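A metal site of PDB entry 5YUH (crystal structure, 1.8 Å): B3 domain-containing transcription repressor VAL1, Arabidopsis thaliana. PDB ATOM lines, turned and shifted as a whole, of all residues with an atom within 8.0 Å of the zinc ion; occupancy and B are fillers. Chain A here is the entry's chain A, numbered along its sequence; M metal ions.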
ATOM      1  N   MET A  10      34.825 -12.504 -29.696  1.00  0.00           N
ATOM      2  CA  MET A  10      34.230 -13.606 -30.444  1.00  0.00           C
ATOM      3  C   MET A  10      33.585 -14.520 -29.409  1.00  0.00           C
ATOM      4  O   MET A  10      34.191 -14.794 -28.368  1.00  0.00           O
ATOM      5  CB  MET A  10      35.278 -14.358 -31.261  1.00  0.00           C
ATOM      6  CG  MET A  10      34.715 -15.305 -32.285  1.00  0.00           C
ATOM      7  SD  MET A  10      35.952 -16.392 -33.034  1.00  0.00           S
ATOM      8  CE  MET A  10      35.390 -16.426 -34.746  1.00  0.00           C
ATOM      9  N   CYS A  11      32.360 -14.956 -29.684  1.00  0.00           N
ATOM     10  CA  CYS A  11      31.666 -15.853 -28.775  1.00  0.00           C
ATOM     11  C   CYS A  11      32.426 -17.165 -28.652  1.00  0.00           C
ATOM     12  O   CYS A  11      32.729 -17.807 -29.661  1.00  0.00           O
ATOM     13  CB  CYS A  11      30.239 -16.097 -29.251  1.00  0.00           C
ATOM     14  SG  CYS A  11      29.367 -17.373 -28.287  1.00  0.00           S
ATOM     15  N   MET A  12      32.704 -17.571 -27.410  1.00  0.00           N
ATOM     16  CA  MET A  12      33.557 -18.727 -27.160  1.00  0.00           C
ATOM     17  C   MET A  12      32.785 -20.041 -27.160  1.00  0.00           C
ATOM     18  O   MET A  12      33.351 -21.089 -26.808  1.00  0.00           O
ATOM     19  CB  MET A  12      34.316 -18.506 -25.847  1.00  0.00           C
ATOM     20  CG  MET A  12      35.322 -17.361 -25.976  1.00  0.00           C
ATOM     21  SD  MET A  12      36.253 -16.957 -24.497  1.00  0.00           S
ATOM     22  CE  MET A  12      37.566 -15.949 -25.208  1.00  0.00           C
ATOM     23  N   ASN A  13      31.529 -20.032 -27.591  1.00  0.00           N
ATOM     24  CA  ASN A  13      30.801 -21.252 -27.929  1.00  0.00           C
ATOM     25  C   ASN A  13      31.242 -21.693 -29.316  1.00  0.00           C
ATOM     26  O   ASN A  13      30.970 -21.007 -30.308  1.00  0.00           O
ATOM     27  CB  ASN A  13      29.296 -21.005 -27.870  1.00  0.00           C
ATOM     28  CG  ASN A  13      28.482 -22.255 -28.187  1.00  0.00           C
ATOM     29  OD1 ASN A  13      29.000 -23.387 -28.194  1.00  0.00           O
ATOM     30  ND2 ASN A  13      27.198 -22.052 -28.448  1.00  0.00           N
ATOM     31  N   ALA A  14      31.929 -22.837 -29.387  1.00  0.00           N
ATOM     32  CA  ALA A  14      32.560 -23.259 -30.642  1.00  0.00           C
ATOM     33  C   ALA A  14      31.555 -23.404 -31.779  1.00  0.00           C
ATOM     34  O   ALA A  14      31.845 -23.062 -32.932  1.00  0.00           O
ATOM     35  CB  ALA A  14      33.327 -24.558 -30.417  1.00  0.00           C
ATOM     36  N   SER A  15      30.360 -23.943 -31.491  1.00  0.00           N
ATOM     37  CA  SER A  15      29.325 -24.060 -32.516  1.00  0.00           C
ATOM     38  C   SER A  15      28.790 -22.700 -32.962  1.00  0.00           C
ATOM     39  O   SER A  15      28.064 -22.644 -33.959  1.00  0.00           O
ATOM     40  CB  SER A  15      28.172 -24.931 -32.007  1.00  0.00           C
ATOM     41  OG  SER A  15      27.596 -24.338 -30.863  1.00  0.00           O
ATOM     42  N   CYS A  16      29.112 -21.630 -32.251  1.00  0.00           N
ATOM     43  CA  CYS A  16      28.625 -20.300 -32.616  1.00  0.00           C
ATOM     44  C   CYS A  16      29.758 -19.456 -33.190  1.00  0.00           C
ATOM     45  O   CYS A  16      29.916 -19.356 -34.409  1.00  0.00           O
ATOM     46  CB  CYS A  16      27.985 -19.616 -31.402  1.00  0.00           C
ATOM     47  SG  CYS A  16      27.487 -17.919 -31.692  1.00  0.00           S
ATOM     48  N   GLY A  17      30.556 -18.853 -32.305  1.00  0.00           N
ATOM     49  CA  GLY A  17      31.709 -18.098 -32.743  1.00  0.00           C
ATOM     50  C   GLY A  17      31.403 -16.807 -33.477  1.00  0.00           C
ATOM     51  O   GLY A  17      32.253 -16.322 -34.235  1.00  0.00           O
ATOM     52  N   THR A  18      30.212 -16.232 -33.282  1.00  0.00           N
ATOM     53  CA  THR A  18      29.898 -14.959 -33.901  1.00  0.00           C
ATOM     54  C   THR A  18      30.791 -13.848 -33.357  1.00  0.00           C
ATOM     55  O   THR A  18      31.328 -13.935 -32.239  1.00  0.00           O
ATOM     56  CB  THR A  18      28.431 -14.571 -33.655  1.00  0.00           C
ATOM     57  OG1 THR A  18      28.138 -13.342 -34.335  1.00  0.00           O
ATOM     58  CG2 THR A  18      28.178 -14.385 -32.159  1.00  0.00           C
ATOM     59  N   THR A  19      30.941 -12.799 -34.164  1.00  0.00           N
ATOM     60  CA  THR A  19      31.577 -11.547 -33.753  1.00  0.00           C
ATOM     61  C   THR A  19      30.596 -10.396 -33.687  1.00  0.00           C
ATOM     62  O   THR A  19      30.992  -9.275 -33.355  1.00  0.00           O
ATOM     63  CB  THR A  19      32.709 -11.191 -34.731  1.00  0.00           C
ATOM     64  OG1 THR A  19      32.237 -11.325 -36.074  1.00  0.00           O
ATOM     65  CG2 THR A  19      33.921 -12.095 -34.510  1.00  0.00           C
ATOM     66  N   SER A  20      29.319 -10.632 -34.011  1.00  0.00           N
ATOM     67  CA  SER A  20      28.282  -9.616 -33.945  1.00  0.00           C
ATOM     68  C   SER A  20      27.133 -10.141 -33.090  1.00  0.00           C
ATOM     69  O   SER A  20      26.635 -11.250 -33.327  1.00  0.00           O
ATOM     70  CB  SER A  20      27.789  -9.213 -35.341  1.00  0.00           C
ATOM     71  OG  SER A  20      27.537 -10.356 -36.134  1.00  0.00           O
ATOM     72  N   THR A  21      26.739  -9.357 -32.094  1.00  0.00           N
ATOM     73  CA  THR A  21      25.622  -9.713 -31.236  1.00  0.00           C
ATOM     74  C   THR A  21      25.044  -8.422 -30.671  1.00  0.00           C
ATOM     75  O   THR A  21      25.734  -7.396 -30.585  1.00  0.00           O
ATOM     76  CB  THR A  21      26.033 -10.652 -30.088  1.00  0.00           C
ATOM     77  OG1 THR A  21      24.875 -11.055 -29.345  1.00  0.00           O
ATOM     78  CG2 THR A  21      27.000  -9.942 -29.156  1.00  0.00           C
ATOM     79  N   TRP A  24      27.032  -8.479 -25.574  1.00  0.00           N
ATOM     80  CA  TRP A  24      28.005  -9.455 -25.104  1.00  0.00           C
ATOM     81  C   TRP A  24      27.701  -9.869 -23.660  1.00  0.00           C
ATOM     82  O   TRP A  24      27.198  -9.077 -22.859  1.00  0.00           O
ATOM     83  CB  TRP A  24      29.435  -8.905 -25.183  1.00  0.00           C
ATOM     84  CG  TRP A  24      29.898  -8.740 -26.599  1.00  0.00           C
ATOM     85  CD1 TRP A  24      30.065  -7.570 -27.269  1.00  0.00           C
ATOM     86  CD2 TRP A  24      30.216  -9.796 -27.523  1.00  0.00           C
ATOM     87  NE1 TRP A  24      30.477  -7.821 -28.566  1.00  0.00           N
ATOM     88  CE2 TRP A  24      30.577  -9.186 -28.740  1.00  0.00           C
ATOM     89  CE3 TRP A  24      30.233 -11.198 -27.445  1.00  0.00           C
ATOM     90  CZ2 TRP A  24      30.958  -9.911 -29.871  1.00  0.00           C
ATOM     91  CZ3 TRP A  24      30.609 -11.927 -28.569  1.00  0.00           C
ATOM     92  CH2 TRP A  24      30.966 -11.288 -29.774  1.00  0.00           C
ATOM     93  N   ASP A  37      33.884 -15.060 -23.009  1.00  0.00           N
ATOM     94  CA  ASP A  37      32.923 -14.187 -23.692  1.00  0.00           C
ATOM     95  C   ASP A  37      31.918 -15.011 -24.486  1.00  0.00           C
ATOM     96  O   ASP A  37      32.306 -15.876 -25.282  1.00  0.00           O
ATOM     97  CB  ASP A  37      33.632 -13.218 -24.644  1.00  0.00           C
ATOM     98  CG  ASP A  37      34.500 -12.204 -23.920  1.00  0.00           C
ATOM     99  OD1 ASP A  37      34.047 -11.627 -22.911  1.00  0.00           O
ATOM    100  OD2 ASP A  37      35.644 -11.993 -24.381  1.00  0.00           O
ATOM    101  N   LEU A  38      30.633 -14.710 -24.296  1.00  0.00           N
ATOM    102  CA  LEU A  38      29.540 -15.342 -25.025  1.00  0.00           C
ATOM    103  C   LEU A  38      28.634 -14.282 -25.642  1.00  0.00           C
ATOM    104  O   LEU A  38      28.450 -13.197 -25.082  1.00  0.00           O
ATOM    105  CB  LEU A  38      28.734 -16.246 -24.102  1.00  0.00           C
ATOM    106  CG  LEU A  38      29.571 -17.360 -23.478  1.00  0.00           C
ATOM    107  CD1 LEU A  38      28.759 -18.128 -22.477  1.00  0.00           C
ATOM    108  CD2 LEU A  38      30.069 -18.263 -24.585  1.00  0.00           C
ATOM    109  N   CYS A  39      28.063 -14.610 -26.811  1.00  0.00           N
ATOM    110  CA  CYS A  39      27.092 -13.712 -27.423  1.00  0.00           C
ATOM    111  C   CYS A  39      25.818 -13.686 -26.589  1.00  0.00           C
ATOM    112  O   CYS A  39      25.674 -14.407 -25.598  1.00  0.00           O
ATOM    113  CB  CYS A  39      26.789 -14.120 -28.860  1.00  0.00           C
ATOM    114  SG  CYS A  39      25.911 -15.677 -29.025  1.00  0.00           S
ATOM    115  N   TYR A  40      24.866 -12.831 -26.978  1.00  0.00           N
ATOM    116  CA  TYR A  40      23.640 -12.718 -26.186  1.00  0.00           C
ATOM    117  C   TYR A  40      22.920 -14.065 -26.091  1.00  0.00           C
ATOM    118  O   TYR A  40      22.430 -14.442 -25.020  1.00  0.00           O
ATOM    119  CB  TYR A  40      22.738 -11.647 -26.795  1.00  0.00           C
ATOM    120  CG  TYR A  40      21.395 -11.529 -26.102  1.00  0.00           C
ATOM    121  CD1 TYR A  40      21.272 -10.892 -24.875  1.00  0.00           C
ATOM    122  CD2 TYR A  40      20.242 -12.076 -26.683  1.00  0.00           C
ATOM    123  CE1 TYR A  40      20.036 -10.783 -24.234  1.00  0.00           C
ATOM    124  CE2 TYR A  40      19.011 -11.983 -26.060  1.00  0.00           C
ATOM    125  CZ  TYR A  40      18.914 -11.334 -24.836  1.00  0.00           C
ATOM    126  OH  TYR A  40      17.683 -11.241 -24.213  1.00  0.00           O
ATOM    127  N   ARG A  41      22.882 -14.812 -27.193  1.00  0.00           N
ATOM    128  CA  ARG A  41      22.150 -16.083 -27.209  1.00  0.00           C
ATOM    129  C   ARG A  41      22.850 -17.140 -26.361  1.00  0.00           C
ATOM    130  O   ARG A  41      22.254 -17.693 -25.409  1.00  0.00           O
ATOM    131  CB  ARG A  41      21.989 -16.548 -28.661  1.00  0.00           C
ATOM    132  CG  ARG A  41      21.175 -17.799 -28.876  1.00  0.00           C
ATOM    133  CD  ARG A  41      21.145 -18.133 -30.358  1.00  0.00           C
ATOM    134  NE  ARG A  41      22.489 -18.464 -30.848  1.00  0.00           N
ATOM    135  CZ  ARG A  41      22.934 -19.703 -31.059  1.00  0.00           C
ATOM    136  NH1 ARG A  41      22.129 -20.748 -30.840  1.00  0.00           N
ATOM    137  NH2 ARG A  41      24.165 -19.894 -31.499  1.00  0.00           N
ATOM    138  N   CYS A  42      24.130 -17.390 -26.645  1.00  0.00           N
ATOM    139  CA  CYS A  42      24.872 -18.390 -25.870  1.00  0.00           C
ATOM    140  C   CYS A  42      25.014 -17.968 -24.413  1.00  0.00           C
ATOM    141  O   CYS A  42      24.852 -18.790 -23.498  1.00  0.00           O
ATOM    142  CB  CYS A  42      26.227 -18.622 -26.523  1.00  0.00           C
ATOM    143  SG  CYS A  42      26.045 -19.231 -28.216  1.00  0.00           S
ATOM    144  N   GLY A  43      25.282 -16.681 -24.171  1.00  0.00           N
ATOM    145  CA  GLY A  43      25.417 -16.213 -22.786  1.00  0.00           C
ATOM    146  C   GLY A  43      24.124 -16.329 -21.997  1.00  0.00           C
ATOM    147  O   GLY A  43      24.148 -16.623 -20.799  1.00  0.00           O
ATOM    148  N   PHE A  51      23.292 -24.277 -20.597  1.00  0.00           N
ATOM    149  CA  PHE A  51      24.214 -24.236 -21.714  1.00  0.00           C
ATOM    150  C   PHE A  51      24.464 -25.635 -22.287  1.00  0.00           C
ATOM    151  O   PHE A  51      24.286 -25.873 -23.493  1.00  0.00           O
ATOM    152  CB  PHE A  51      25.517 -23.568 -21.285  1.00  0.00           C
ATOM    153  CG  PHE A  51      26.485 -23.387 -22.392  1.00  0.00           C
ATOM    154  CD1 PHE A  51      27.417 -24.363 -22.686  1.00  0.00           C
ATOM    155  CD2 PHE A  51      26.467 -22.219 -23.157  1.00  0.00           C
ATOM    156  CE1 PHE A  51      28.313 -24.195 -23.730  1.00  0.00           C
ATOM    157  CE2 PHE A  51      27.347 -22.028 -24.187  1.00  0.00           C
ATOM    158  CZ  PHE A  51      28.283 -23.013 -24.483  1.00  0.00           C
ATOM    159  N   PHE A  55      23.546 -27.045 -26.078  1.00  0.00           N
ATOM    160  CA  PHE A  55      24.591 -27.073 -27.099  1.00  0.00           C
ATOM    161  C   PHE A  55      25.426 -28.339 -27.137  1.00  0.00           C
ATOM    162  O   PHE A  55      26.075 -28.595 -28.154  1.00  0.00           O
ATOM    163  CB  PHE A  55      25.542 -25.888 -26.920  1.00  0.00           C
ATOM    164  CG  PHE A  55      24.889 -24.537 -27.110  1.00  0.00           C
ATOM    165  CD1 PHE A  55      24.486 -24.124 -28.377  1.00  0.00           C
ATOM    166  CD2 PHE A  55      24.682 -23.692 -26.026  1.00  0.00           C
ATOM    167  CE1 PHE A  55      23.888 -22.886 -28.550  1.00  0.00           C
ATOM    168  CE2 PHE A  55      24.083 -22.454 -26.200  1.00  0.00           C
ATOM    169  CZ  PHE A  55      23.681 -22.041 -27.466  1.00  0.00           C
HETATM  170 ZN    ZN M   1      27.268 -17.441 -29.405  1.00  0.00          ZN
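Of the 22 residues printed, 4 come within 4 Å of the zinc ion.
The side-chain sulfur (SG) of Cys 39 sits close to the backbone NH (N) of Arg 41.
The side-chain sulfur (SG) of Cys 16 sits close to the backbone NH (N) of Thr 18 (3.6 Å).
The backbone NH (N) of Cys 11 is in hydrogen-bond range of the backbone carbonyl oxygen (O) of Thr 18, 2.9 Å away.
N of Asn 13 lies close to SG of Cys 11 (3.5 Å).
The side-chain sulfur (SG) of Cys 42 sits close to the side-chain amide nitrogen (ND2) of Asn 13, at 3.1 Å.
The zinc ion is bound by the side-chain sulfur (SG) of Cys 39 (2.3 Å), the side-chain sulfur (SG) of Cys 16 (2.3 Å), the side-chain sulfur (SG) of Cys 11 (2.4 Å) and the side-chain sulfur (SG) of Cys 42 (2.5 Å).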
